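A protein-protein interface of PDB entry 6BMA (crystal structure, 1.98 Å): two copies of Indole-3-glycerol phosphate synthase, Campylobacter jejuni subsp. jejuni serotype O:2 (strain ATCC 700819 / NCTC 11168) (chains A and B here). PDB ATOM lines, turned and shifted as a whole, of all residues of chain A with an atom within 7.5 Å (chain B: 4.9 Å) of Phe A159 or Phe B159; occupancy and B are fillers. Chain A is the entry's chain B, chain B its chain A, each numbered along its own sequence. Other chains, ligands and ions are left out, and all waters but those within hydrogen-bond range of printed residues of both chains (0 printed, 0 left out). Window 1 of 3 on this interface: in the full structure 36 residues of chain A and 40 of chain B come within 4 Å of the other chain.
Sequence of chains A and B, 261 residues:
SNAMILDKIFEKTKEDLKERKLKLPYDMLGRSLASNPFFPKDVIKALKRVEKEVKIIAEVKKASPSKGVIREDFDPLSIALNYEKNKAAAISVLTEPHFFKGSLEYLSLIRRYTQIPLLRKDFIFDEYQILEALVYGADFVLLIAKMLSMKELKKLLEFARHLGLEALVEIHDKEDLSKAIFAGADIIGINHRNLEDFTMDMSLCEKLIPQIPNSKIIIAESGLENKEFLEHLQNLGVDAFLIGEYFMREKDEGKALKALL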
ATOM      1  N   TYR A  26      -1.059 -16.974  -4.966  1.00  0.00           N
ATOM      2  CA  TYR A  26      -1.605 -15.733  -5.510  1.00  0.00           C
ATOM      3  C   TYR A  26      -0.495 -14.819  -6.025  1.00  0.00           C
ATOM      4  O   TYR A  26      -0.592 -14.251  -7.118  1.00  0.00           O
ATOM      5  CB  TYR A  26      -2.409 -14.993  -4.440  1.00  0.00           C
ATOM      6  CG  TYR A  26      -3.902 -15.303  -4.298  1.00  0.00           C
ATOM      7  CD1 TYR A  26      -4.830 -14.822  -5.219  1.00  0.00           C
ATOM      8  CD2 TYR A  26      -4.376 -15.992  -3.190  1.00  0.00           C
ATOM      9  CE1 TYR A  26      -6.203 -15.053  -5.055  1.00  0.00           C
ATOM     10  CE2 TYR A  26      -5.733 -16.247  -3.017  1.00  0.00           C
ATOM     11  CZ  TYR A  26      -6.636 -15.785  -3.947  1.00  0.00           C
ATOM     12  OH  TYR A  26      -7.970 -16.016  -3.741  1.00  0.00           O
ATOM     13  N   ASP A 126      -9.357   2.908  -5.405  1.00  0.00           N
ATOM     14  CA  ASP A 126     -10.218   2.174  -6.328  1.00  0.00           C
ATOM     15  C   ASP A 126      -9.489   0.946  -6.858  1.00  0.00           C
ATOM     16  O   ASP A 126      -8.280   0.994  -7.098  1.00  0.00           O
ATOM     17  CB  ASP A 126     -10.654   3.083  -7.483  1.00  0.00           C
ATOM     18  CG  ASP A 126     -11.672   2.428  -8.385  1.00  0.00           C
ATOM     19  OD1 ASP A 126     -12.707   1.952  -7.874  1.00  0.00           O
ATOM     20  OD2 ASP A 126     -11.437   2.403  -9.605  1.00  0.00           O
ATOM     21  N   GLU A 127     -10.242  -0.147  -7.045  1.00  0.00           N
ATOM     22  CA  GLU A 127      -9.674  -1.400  -7.541  1.00  0.00           C
ATOM     23  C   GLU A 127      -8.915  -1.221  -8.859  1.00  0.00           C
ATOM     24  O   GLU A 127      -7.885  -1.864  -9.083  1.00  0.00           O
ATOM     25  CB  GLU A 127     -10.793  -2.446  -7.697  1.00  0.00           C
ATOM     26  CG  GLU A 127     -11.313  -3.028  -6.364  1.00  0.00           C
ATOM     27  CD  GLU A 127     -12.390  -2.182  -5.686  1.00  0.00           C
ATOM     28  OE1 GLU A 127     -12.601  -1.009  -6.083  1.00  0.00           O
ATOM     29  OE2 GLU A 127     -13.028  -2.701  -4.744  1.00  0.00           O
ATOM     30  N   TYR A 128      -9.412  -0.364  -9.751  1.00  0.00           N
ATOM     31  CA  TYR A 128      -8.734  -0.157 -11.035  1.00  0.00           C
ATOM     32  C   TYR A 128      -7.266   0.236 -10.855  1.00  0.00           C
ATOM     33  O   TYR A 128      -6.389  -0.208 -11.614  1.00  0.00           O
ATOM     34  CB  TYR A 128      -9.480   0.917 -11.827  1.00  0.00           C
ATOM     35  CG  TYR A 128      -8.922   1.213 -13.212  1.00  0.00           C
ATOM     36  CD1 TYR A 128      -7.897   2.157 -13.396  1.00  0.00           C
ATOM     37  CD2 TYR A 128      -9.445   0.579 -14.339  1.00  0.00           C
ATOM     38  CE1 TYR A 128      -7.407   2.442 -14.660  1.00  0.00           C
ATOM     39  CE2 TYR A 128      -8.954   0.866 -15.624  1.00  0.00           C
ATOM     40  CZ  TYR A 128      -7.940   1.791 -15.771  1.00  0.00           C
ATOM     41  OH  TYR A 128      -7.457   2.074 -17.033  1.00  0.00           O
ATOM     42  N   GLN A 129      -6.977   1.091  -9.869  1.00  0.00           N
ATOM     43  CA  GLN A 129      -5.597   1.536  -9.657  1.00  0.00           C
ATOM     44  C   GLN A 129      -4.701   0.403  -9.177  1.00  0.00           C
ATOM     45  O   GLN A 129      -3.491   0.412  -9.434  1.00  0.00           O
ATOM     46  CB  GLN A 129      -5.568   2.666  -8.635  1.00  0.00           C
ATOM     47  CG  GLN A 129      -6.362   3.902  -9.033  1.00  0.00           C
ATOM     48  CD  GLN A 129      -6.521   4.825  -7.854  1.00  0.00           C
ATOM     49  OE1 GLN A 129      -7.171   4.465  -6.863  1.00  0.00           O
ATOM     50  NE2 GLN A 129      -5.908   6.003  -7.927  1.00  0.00           N
ATOM     51  N   ILE A 130      -5.276  -0.559  -8.460  1.00  0.00           N
ATOM     52  CA  ILE A 130      -4.530  -1.732  -8.008  1.00  0.00           C
ATOM     53  C   ILE A 130      -4.326  -2.726  -9.154  1.00  0.00           C
ATOM     54  O   ILE A 130      -3.264  -3.345  -9.273  1.00  0.00           O
ATOM     55  CB  ILE A 130      -5.264  -2.367  -6.806  1.00  0.00           C
ATOM     56  CG1 ILE A 130      -5.292  -1.381  -5.627  1.00  0.00           C
ATOM     57  CG2 ILE A 130      -4.604  -3.687  -6.385  1.00  0.00           C
ATOM     58  CD1 ILE A 130      -6.241  -1.841  -4.458  1.00  0.00           C
ATOM     59  N   LEU A 131      -5.325  -2.903 -10.019  1.00  0.00           N
ATOM     60  CA  LEU A 131      -5.090  -3.691 -11.226  1.00  0.00           C
ATOM     61  C   LEU A 131      -4.008  -3.053 -12.092  1.00  0.00           C
ATOM     62  O   LEU A 131      -3.146  -3.754 -12.646  1.00  0.00           O
ATOM     63  CB  LEU A 131      -6.391  -3.853 -12.023  1.00  0.00           C
ATOM     64  CG  LEU A 131      -6.298  -4.702 -13.299  1.00  0.00           C
ATOM     65  CD1 LEU A 131      -5.780  -6.103 -12.975  1.00  0.00           C
ATOM     66  CD2 LEU A 131      -7.666  -4.785 -13.989  1.00  0.00           C
ATOM     67  N   GLU A 132      -4.041  -1.724 -12.232  1.00  0.00           N
ATOM     68  CA  GLU A 132      -2.944  -0.999 -12.883  1.00  0.00           C
ATOM     69  C   GLU A 132      -1.596  -1.355 -12.275  1.00  0.00           C
ATOM     70  O   GLU A 132      -0.613  -1.602 -12.990  1.00  0.00           O
ATOM     71  CB  GLU A 132      -3.148   0.513 -12.746  1.00  0.00           C
ATOM     72  CG  GLU A 132      -4.120   1.122 -13.722  1.00  0.00           C
ATOM     73  CD  GLU A 132      -4.163   2.637 -13.570  1.00  0.00           C
ATOM     74  OE1 GLU A 132      -4.142   3.116 -12.410  1.00  0.00           O
ATOM     75  OE2 GLU A 132      -4.183   3.335 -14.612  1.00  0.00           O
ATOM     76  N   LEU A 134      -0.666  -3.971 -10.679  1.00  0.00           N
ATOM     77  CA  LEU A 134      -0.296  -5.330 -11.087  1.00  0.00           C
ATOM     78  C   LEU A 134       0.286  -5.361 -12.500  1.00  0.00           C
ATOM     79  O   LEU A 134       1.394  -5.870 -12.725  1.00  0.00           O
ATOM     80  CB  LEU A 134      -1.516  -6.263 -11.023  1.00  0.00           C
ATOM     81  CG  LEU A 134      -1.252  -7.681 -11.527  1.00  0.00           C
ATOM     82  CD1 LEU A 134      -0.194  -8.343 -10.680  1.00  0.00           C
ATOM     83  CD2 LEU A 134      -2.537  -8.525 -11.549  1.00  0.00           C
ATOM     84  N   LEU A 153     -10.626   0.437   3.240  1.00  0.00           N
ATOM     85  CA  LEU A 153      -9.234   0.009   3.346  1.00  0.00           C
ATOM     86  C   LEU A 153      -9.121  -1.510   3.296  1.00  0.00           C
ATOM     87  O   LEU A 153      -8.254  -2.048   2.599  1.00  0.00           O
ATOM     88  CB  LEU A 153      -8.622   0.546   4.640  1.00  0.00           C
ATOM     89  CG  LEU A 153      -7.191   0.099   4.924  1.00  0.00           C
ATOM     90  CD1 LEU A 153      -6.273   0.536   3.798  1.00  0.00           C
ATOM     91  CD2 LEU A 153      -6.718   0.643   6.266  1.00  0.00           C
ATOM     92  N   LYS A 154      -9.986  -2.218   4.031  1.00  0.00           N
ATOM     93  CA  LYS A 154      -9.957  -3.677   3.994  1.00  0.00           C
ATOM     94  C   LYS A 154     -10.329  -4.205   2.613  1.00  0.00           C
ATOM     95  O   LYS A 154      -9.696  -5.144   2.107  1.00  0.00           O
ATOM     96  CB  LYS A 154     -10.887  -4.259   5.054  1.00  0.00           C
ATOM     97  CG  LYS A 154     -10.936  -5.783   5.014  1.00  0.00           C
ATOM     98  CD  LYS A 154     -11.785  -6.324   6.139  1.00  0.00           C
ATOM     99  CE  LYS A 154     -11.903  -7.835   6.056  1.00  0.00           C
ATOM    100  NZ  LYS A 154     -12.684  -8.328   7.212  1.00  0.00           N
ATOM    101  N   LYS A 155     -11.335  -3.602   1.978  1.00  0.00           N
ATOM    102  CA  LYS A 155     -11.703  -4.008   0.624  1.00  0.00           C
ATOM    103  C   LYS A 155     -10.527  -3.881  -0.342  1.00  0.00           C
ATOM    104  O   LYS A 155     -10.278  -4.776  -1.163  1.00  0.00           O
ATOM    105  CB  LYS A 155     -12.879  -3.170   0.124  1.00  0.00           C
ATOM    106  CG  LYS A 155     -13.462  -3.687  -1.174  1.00  0.00           C
ATOM    107  CD  LYS A 155     -14.695  -2.904  -1.561  1.00  0.00           C
ATOM    108  CE  LYS A 155     -14.314  -1.509  -2.019  1.00  0.00           C
ATOM    109  NZ  LYS A 155     -15.506  -0.672  -2.333  1.00  0.00           N
ATOM    110  N   LEU A 156      -9.810  -2.757  -0.295  1.00  0.00           N
ATOM    111  CA  LEU A 156      -8.726  -2.566  -1.256  1.00  0.00           C
ATOM    112  C   LEU A 156      -7.526  -3.436  -0.910  1.00  0.00           C
ATOM    113  O   LEU A 156      -6.831  -3.931  -1.806  1.00  0.00           O
ATOM    114  CB  LEU A 156      -8.326  -1.087  -1.323  1.00  0.00           C
ATOM    115  CG  LEU A 156      -9.439  -0.129  -1.770  1.00  0.00           C
ATOM    116  CD1 LEU A 156      -9.052   1.324  -1.480  1.00  0.00           C
ATOM    117  CD2 LEU A 156      -9.772  -0.311  -3.252  1.00  0.00           C
ATOM    118  N   LEU A 157      -7.254  -3.624   0.380  1.00  0.00           N
ATOM    119  CA  LEU A 157      -6.165  -4.513   0.767  1.00  0.00           C
ATOM    120  C   LEU A 157      -6.447  -5.943   0.314  1.00  0.00           C
ATOM    121  O   LEU A 157      -5.547  -6.640  -0.178  1.00  0.00           O
ATOM    122  CB  LEU A 157      -5.947  -4.458   2.285  1.00  0.00           C
ATOM    123  CG  LEU A 157      -4.694  -5.190   2.787  1.00  0.00           C
ATOM    124  CD1 LEU A 157      -4.011  -4.422   3.918  1.00  0.00           C
ATOM    125  CD2 LEU A 157      -5.006  -6.620   3.226  1.00  0.00           C
ATOM    126  N   GLU A 158      -7.693  -6.394   0.466  1.00  0.00           N
ATOM    127  CA  GLU A 158      -8.045  -7.742   0.032  1.00  0.00           C
ATOM    128  C   GLU A 158      -7.937  -7.882  -1.483  1.00  0.00           C
ATOM    129  O   GLU A 158      -7.458  -8.909  -1.988  1.00  0.00           O
ATOM    130  CB  GLU A 158      -9.454  -8.088   0.506  1.00  0.00           C
ATOM    131  CG  GLU A 158      -9.525  -8.414   1.985  1.00  0.00           C
ATOM    132  CD  GLU A 158      -8.868  -9.743   2.298  1.00  0.00           C
ATOM    133  OE1 GLU A 158      -9.449 -10.786   1.934  1.00  0.00           O
ATOM    134  OE2 GLU A 158      -7.759  -9.737   2.873  1.00  0.00           O
ATOM    135  N   PHE A 159      -8.405  -6.879  -2.221  1.00  0.00           N
ATOM    136  CA  PHE A 159      -8.267  -6.912  -3.670  1.00  0.00           C
ATOM    137  C   PHE A 159      -6.803  -6.982  -4.089  1.00  0.00           C
ATOM    138  O   PHE A 159      -6.445  -7.750  -4.993  1.00  0.00           O
ATOM    139  CB  PHE A 159      -8.935  -5.698  -4.301  1.00  0.00           C
ATOM    140  CG  PHE A 159      -8.934  -5.744  -5.803  1.00  0.00           C
ATOM    141  CD1 PHE A 159      -9.776  -6.626  -6.478  1.00  0.00           C
ATOM    142  CD2 PHE A 159      -8.088  -4.926  -6.537  1.00  0.00           C
ATOM    143  CE1 PHE A 159      -9.772  -6.697  -7.863  1.00  0.00           C
ATOM    144  CE2 PHE A 159      -8.083  -4.983  -7.923  1.00  0.00           C
ATOM    145  CZ  PHE A 159      -8.931  -5.859  -8.589  1.00  0.00           C
ATOM    146  N   ALA A 160      -5.938  -6.183  -3.458  1.00  0.00           N
ATOM    147  CA  ALA A 160      -4.512  -6.282  -3.751  1.00  0.00           C
ATOM    148  C   ALA A 160      -4.012  -7.690  -3.462  1.00  0.00           C
ATOM    149  O   ALA A 160      -3.297  -8.294  -4.275  1.00  0.00           O
ATOM    150  CB  ALA A 160      -3.717  -5.236  -2.946  1.00  0.00           C
ATOM    151  N   ARG A 161      -4.396  -8.237  -2.308  1.00  0.00           N
ATOM    152  CA  ARG A 161      -3.959  -9.579  -1.951  1.00  0.00           C
ATOM    153  C   ARG A 161      -4.437 -10.604  -2.979  1.00  0.00           C
ATOM    154  O   ARG A 161      -3.693 -11.526  -3.343  1.00  0.00           O
ATOM    155  CB  ARG A 161      -4.460  -9.938  -0.550  1.00  0.00           C
ATOM    156  CG  ARG A 161      -4.032 -11.328  -0.095  1.00  0.00           C
ATOM    157  CD  ARG A 161      -4.492 -11.678   1.334  1.00  0.00           C
ATOM    158  NE  ARG A 161      -5.937 -11.870   1.443  1.00  0.00           N
ATOM    159  CZ  ARG A 161      -6.598 -12.988   1.130  1.00  0.00           C
ATOM    160  NH1 ARG A 161      -5.965 -14.066   0.665  1.00  0.00           N
ATOM    161  NH2 ARG A 161      -7.912 -13.030   1.288  1.00  0.00           N
ATOM    162  N   HIS A 162      -5.667 -10.447  -3.470  1.00  0.00           N
ATOM    163  CA  HIS A 162      -6.214 -11.370  -4.459  1.00  0.00           C
ATOM    164  C   HIS A 162      -5.599 -11.201  -5.850  1.00  0.00           C
ATOM    165  O   HIS A 162      -5.871 -12.037  -6.724  1.00  0.00           O
ATOM    166  CB  HIS A 162      -7.727 -11.191  -4.540  1.00  0.00           C
ATOM    167  CG  HIS A 162      -8.467 -11.765  -3.369  1.00  0.00           C
ATOM    168  ND1 HIS A 162      -9.602 -11.182  -2.850  1.00  0.00           N
ATOM    169  CD2 HIS A 162      -8.246 -12.879  -2.633  1.00  0.00           C
ATOM    170  CE1 HIS A 162     -10.050 -11.913  -1.845  1.00  0.00           C
ATOM    171  NE2 HIS A 162      -9.243 -12.950  -1.693  1.00  0.00           N
ATOM    172  N   LEU A 163      -4.809 -10.148  -6.083  1.00  0.00           N
ATOM    173  CA  LEU A 163      -3.985 -10.024  -7.283  1.00  0.00           C
ATOM    174  C   LEU A 163      -2.553 -10.459  -7.035  1.00  0.00           C
ATOM    175  O   LEU A 163      -1.730 -10.419  -7.955  1.00  0.00           O
ATOM    176  CB  LEU A 163      -3.974  -8.579  -7.812  1.00  0.00           C
ATOM    177  CG  LEU A 163      -5.285  -7.925  -8.264  1.00  0.00           C
ATOM    178  CD1 LEU A 163      -5.061  -6.689  -9.151  1.00  0.00           C
ATOM    179  CD2 LEU A 163      -6.178  -8.882  -8.946  1.00  0.00           C
ATOM    180  N   GLY A 164      -2.237 -10.847  -5.810  1.00  0.00           N
ATOM    181  CA  GLY A 164      -0.884 -11.208  -5.475  1.00  0.00           C
ATOM    182  C   GLY A 164      -0.009 -10.046  -5.087  1.00  0.00           C
ATOM    183  O   GLY A 164       1.218 -10.187  -5.088  1.00  0.00           O
ATOM    184  N   LEU A 165      -0.592  -8.894  -4.767  1.00  0.00           N
ATOM    185  CA  LEU A 165       0.177  -7.725  -4.353  1.00  0.00           C
ATOM    186  C   LEU A 165       0.081  -7.541  -2.844  1.00  0.00           C
ATOM    187  O   LEU A 165      -0.982  -7.730  -2.257  1.00  0.00           O
ATOM    188  CB  LEU A 165      -0.327  -6.462  -5.048  1.00  0.00           C
ATOM    189  CG  LEU A 165      -0.366  -6.518  -6.570  1.00  0.00           C
ATOM    190  CD1 LEU A 165      -0.926  -5.219  -7.120  1.00  0.00           C
ATOM    191  CD2 LEU A 165       1.026  -6.773  -7.101  1.00  0.00           C
ATOM    192  N   GLU B 127     -11.714 -16.226  -5.279  1.00  0.00           N
ATOM    193  CA  GLU B 127     -11.128 -15.221  -6.166  1.00  0.00           C
ATOM    194  C   GLU B 127      -9.958 -15.783  -6.970  1.00  0.00           C
ATOM    195  O   GLU B 127      -9.758 -15.409  -8.132  1.00  0.00           O
ATOM    196  CB  GLU B 127     -10.693 -14.013  -5.335  1.00  0.00           C
ATOM    197  CG  GLU B 127     -11.848 -13.167  -4.828  1.00  0.00           C
ATOM    198  CD  GLU B 127     -12.458 -13.640  -3.502  1.00  0.00           C
ATOM    199  OE1 GLU B 127     -12.226 -14.787  -3.051  1.00  0.00           O
ATOM    200  OE2 GLU B 127     -13.200 -12.841  -2.904  1.00  0.00           O
ATOM    201  N   ILE B 130     -10.884 -17.019 -10.300  1.00  0.00           N
ATOM    202  CA  ILE B 130     -11.187 -15.964 -11.261  1.00  0.00           C
ATOM    203  C   ILE B 130      -9.902 -15.300 -11.759  1.00  0.00           C
ATOM    204  O   ILE B 130      -9.785 -14.958 -12.942  1.00  0.00           O
ATOM    205  CB  ILE B 130     -12.176 -14.967 -10.621  1.00  0.00           C
ATOM    206  CG1 ILE B 130     -13.478 -15.695 -10.256  1.00  0.00           C
ATOM    207  CG2 ILE B 130     -12.450 -13.778 -11.559  1.00  0.00           C
ATOM    208  CD1 ILE B 130     -14.501 -14.848  -9.512  1.00  0.00           C
ATOM    209  N   LEU B 131      -8.904 -15.134 -10.890  1.00  0.00           N
ATOM    210  CA  LEU B 131      -7.604 -14.670 -11.379  1.00  0.00           C
ATOM    211  C   LEU B 131      -6.994 -15.679 -12.350  1.00  0.00           C
ATOM    212  O   LEU B 131      -6.425 -15.293 -13.378  1.00  0.00           O
ATOM    213  CB  LEU B 131      -6.654 -14.397 -10.210  1.00  0.00           C
ATOM    214  CG  LEU B 131      -5.239 -13.917 -10.567  1.00  0.00           C
ATOM    215  CD1 LEU B 131      -5.276 -12.564 -11.314  1.00  0.00           C
ATOM    216  CD2 LEU B 131      -4.396 -13.792  -9.299  1.00  0.00           C
ATOM    217  N   LYS B 155     -19.833 -10.732  -4.300  1.00  0.00           N
ATOM    218  CA  LYS B 155     -18.393 -10.527  -4.172  1.00  0.00           C
ATOM    219  C   LYS B 155     -17.638 -11.092  -5.367  1.00  0.00           C
ATOM    220  O   LYS B 155     -16.727 -10.444  -5.903  1.00  0.00           O
ATOM    221  CB  LYS B 155     -17.902 -11.158  -2.868  1.00  0.00           C
ATOM    222  CG  LYS B 155     -16.408 -11.108  -2.680  1.00  0.00           C
ATOM    223  CD  LYS B 155     -16.031 -11.521  -1.269  1.00  0.00           C
ATOM    224  CE  LYS B 155     -16.034 -13.028  -1.114  1.00  0.00           C
ATOM    225  NZ  LYS B 155     -15.778 -13.424   0.304  1.00  0.00           N
ATOM    226  N   LEU B 156     -18.012 -12.290  -5.823  1.00  0.00           N
ATOM    227  CA  LEU B 156     -17.281 -12.899  -6.930  1.00  0.00           C
ATOM    228  C   LEU B 156     -17.591 -12.200  -8.244  1.00  0.00           C
ATOM    229  O   LEU B 156     -16.698 -12.015  -9.080  1.00  0.00           O
ATOM    230  CB  LEU B 156     -17.603 -14.396  -7.019  1.00  0.00           C
ATOM    231  CG  LEU B 156     -17.131 -15.183  -5.798  1.00  0.00           C
ATOM    232  CD1 LEU B 156     -17.647 -16.621  -5.807  1.00  0.00           C
ATOM    233  CD2 LEU B 156     -15.617 -15.170  -5.717  1.00  0.00           C
ATOM    234  N   LEU B 157     -18.856 -11.813  -8.446  1.00  0.00           N
ATOM    235  CA  LEU B 157     -19.209 -11.000  -9.602  1.00  0.00           C
ATOM    236  C   LEU B 157     -18.390  -9.722  -9.634  1.00  0.00           C
ATOM    237  O   LEU B 157     -17.895  -9.320 -10.694  1.00  0.00           O
ATOM    238  CB  LEU B 157     -20.697 -10.651  -9.587  1.00  0.00           C
ATOM    239  CG  LEU B 157     -21.708 -11.716 -10.004  1.00  0.00           C
ATOM    240  CD1 LEU B 157     -23.128 -11.218  -9.777  1.00  0.00           C
ATOM    241  CD2 LEU B 157     -21.510 -12.096 -11.451  1.00  0.00           C
ATOM    242  N   GLU B 158     -18.240  -9.076  -8.474  1.00  0.00           N
ATOM    243  CA  GLU B 158     -17.509  -7.819  -8.392  1.00  0.00           C
ATOM    244  C   GLU B 158     -16.026  -8.034  -8.661  1.00  0.00           C
ATOM    245  O   GLU B 158     -15.394  -7.229  -9.358  1.00  0.00           O
ATOM    246  CB  GLU B 158     -17.725  -7.178  -7.021  1.00  0.00           C
ATOM    247  CG  GLU B 158     -19.040  -6.413  -6.884  1.00  0.00           C
ATOM    248  CD  GLU B 158     -19.098  -5.212  -7.813  1.00  0.00           C
ATOM    249  OE1 GLU B 158     -18.434  -4.192  -7.516  1.00  0.00           O
ATOM    250  OE2 GLU B 158     -19.787  -5.292  -8.853  1.00  0.00           O
ATOM    251  N   PHE B 159     -15.450  -9.099  -8.100  1.00  0.00           N
ATOM    252  CA  PHE B 159     -14.054  -9.417  -8.387  1.00  0.00           C
ATOM    253  C   PHE B 159     -13.841  -9.658  -9.881  1.00  0.00           C
ATOM    254  O   PHE B 159     -12.892  -9.129 -10.480  1.00  0.00           O
ATOM    255  CB  PHE B 159     -13.596 -10.630  -7.562  1.00  0.00           C
ATOM    256  CG  PHE B 159     -12.110 -10.875  -7.643  1.00  0.00           C
ATOM    257  CD1 PHE B 159     -11.222  -9.981  -7.054  1.00  0.00           C
ATOM    258  CD2 PHE B 159     -11.597 -11.981  -8.320  1.00  0.00           C
ATOM    259  CE1 PHE B 159      -9.850 -10.175  -7.135  1.00  0.00           C
ATOM    260  CE2 PHE B 159     -10.214 -12.192  -8.401  1.00  0.00           C
ATOM    261  CZ  PHE B 159      -9.339 -11.276  -7.804  1.00  0.00           C
ATOM    262  N   ALA B 160     -14.727 -10.439 -10.506  1.00  0.00           N
ATOM    263  CA  ALA B 160     -14.641 -10.660 -11.950  1.00  0.00           C
ATOM    264  C   ALA B 160     -14.677  -9.333 -12.706  1.00  0.00           C
ATOM    265  O   ALA B 160     -13.811  -9.061 -13.552  1.00  0.00           O
ATOM    266  CB  ALA B 160     -15.777 -11.596 -12.416  1.00  0.00           C
ATOM    267  N   ARG B 161     -15.629  -8.461 -12.357  1.00  0.00           N
ATOM    268  CA  ARG B 161     -15.741  -7.173 -13.035  1.00  0.00           C
ATOM    269  C   ARG B 161     -14.471  -6.341 -12.859  1.00  0.00           C
ATOM    270  O   ARG B 161     -14.017  -5.674 -13.799  1.00  0.00           O
ATOM    271  CB  ARG B 161     -16.962  -6.410 -12.515  1.00  0.00           C
ATOM    272  CG  ARG B 161     -17.214  -5.098 -13.229  1.00  0.00           C
ATOM    273  CD  ARG B 161     -18.422  -4.297 -12.693  1.00  0.00           C
ATOM    274  NE  ARG B 161     -18.292  -3.837 -11.303  1.00  0.00           N
ATOM    275  CZ  ARG B 161     -17.667  -2.723 -10.915  1.00  0.00           C
ATOM    276  NH1 ARG B 161     -17.070  -1.927 -11.799  1.00  0.00           N
ATOM    277  NH2 ARG B 161     -17.631  -2.400  -9.627  1.00  0.00           N
ATOM    278  N   HIS B 162     -13.875  -6.376 -11.665  1.00  0.00           N
ATOM    279  CA  HIS B 162     -12.664  -5.602 -11.409  1.00  0.00           C
ATOM    280  C   HIS B 162     -11.421  -6.197 -12.062  1.00  0.00           C
ATOM    281  O   HIS B 162     -10.366  -5.550 -12.041  1.00  0.00           O
ATOM    282  CB  HIS B 162     -12.416  -5.471  -9.897  1.00  0.00           C
ATOM    283  CG  HIS B 162     -13.365  -4.549  -9.195  1.00  0.00           C
ATOM    284  ND1 HIS B 162     -13.853  -4.814  -7.934  1.00  0.00           N
ATOM    285  CD2 HIS B 162     -13.907  -3.363  -9.568  1.00  0.00           C
ATOM    286  CE1 HIS B 162     -14.648  -3.825  -7.554  1.00  0.00           C
ATOM    287  NE2 HIS B 162     -14.699  -2.935  -8.529  1.00  0.00           N
ATOM    288  N   LEU B 163     -11.493  -7.414 -12.597  1.00  0.00           N
ATOM    289  CA  LEU B 163     -10.443  -7.962 -13.447  1.00  0.00           C
ATOM    290  C   LEU B 163     -10.737  -7.786 -14.926  1.00  0.00           C
ATOM    291  O   LEU B 163      -9.922  -8.196 -15.755  1.00  0.00           O
ATOM    292  CB  LEU B 163     -10.224  -9.463 -13.174  1.00  0.00           C
ATOM    293  CG  LEU B 163      -9.664  -9.897 -11.817  1.00  0.00           C
ATOM    294  CD1 LEU B 163      -9.133 -11.330 -11.880  1.00  0.00           C
ATOM    295  CD2 LEU B 163      -8.596  -8.972 -11.388  1.00  0.00           C
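A ring nitrogen (ND1) of His B162 is in hydrogen-bond range of the backbone carbonyl oxygen (O) of Glu B158, 3.2 Å away.
NH2 of Arg B161 is in hydrogen-bond range of NE2 of His B162, 3.2 Å away.
The backbone carbonyl oxygen (O) of Glu A158 is in hydrogen-bond range of a ring nitrogen (ND1) of His A162 (3.2 Å).
A ring nitrogen (NE2) of His A162 is in hydrogen-bond range of the guanidinium group (NH2) of Arg A161 (3.3 Å).
Of the 12 printed residues of chain B, 5 touch a printed residue of chain A.
Printed residues of chain B that touch a printed residue of chain A: Glu B127, Leu B131, Phe B159, His B162 and Leu B163.
Along chain B the printed residues that touch a printed residue of chain A span positions 127 to 163.
Printed residues of chain A that touch a printed residue of chain B: Tyr A26, Glu A127, Leu A131, Phe A159, His A162 and Leu A163.
Hydrophobic or aromatic side chains of chain A within 4 Å of the printed part of chain B: Tyr A26, Leu A131, Phe A159, His A162 and Leu A163.
Asp A126 touches none of the printed residues of chain B.
Of the printed residues of chain B, Glu A127 touches His B162.
Of the printed residues of chain B, Leu A131 touches His B162 (3.4 Å).
Phe A159 touches just these residues of chain B: Phe B159 (3.6 Å) and His B162 (3.6 Å).
Of the printed residues of chain B, His A162 touches Glu B127 (3.4 Å), Leu B131 (3.4 Å) and Phe B159 (3.5 Å).
Of the printed residues of chain A, Leu B131 touches His A162.
Phe B159 touches just these residues of chain A: Phe A159 (3.6 Å) and His A162 (3.5 Å).
The nearest residue of chain B that does not touch Phe A159 is Leu B163 (4.2 Å).
The nearest printed residue of chain B that does not touch Tyr A26 is Leu B131 (4.2 Å).
Among the printed residues, merely in contact across the chains: Glu A127 with His B162 (3.4 Å), His A162 with Glu B127 (3.4 Å), Leu A131 with His B162 (3.4 Å), Leu A163 with Leu B163 (3.4 Å), His A162 with Leu B131 (3.4 Å), His A162 with Phe B159 (3.5 Å), Phe A159 with His B162 (3.6 Å), Phe A159 with Phe B159 (3.6 Å) and Tyr A26 with Glu B127 (3.7 Å).
Glu A127 touches His B162, and with the chains exchanged His A162 touches Glu B127.
Leu A131 touches His B162, and with the chains exchanged His A162 touches Leu B131.
Phe A159 touches His B162, and with the chains exchanged His A162 touches Phe B159.
Leu A163 touches its own counterpart, Leu B163.
Of the 9 pairs that touch across the chains among the printed residues, 8 have their exchanged pair printed and touching as well.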
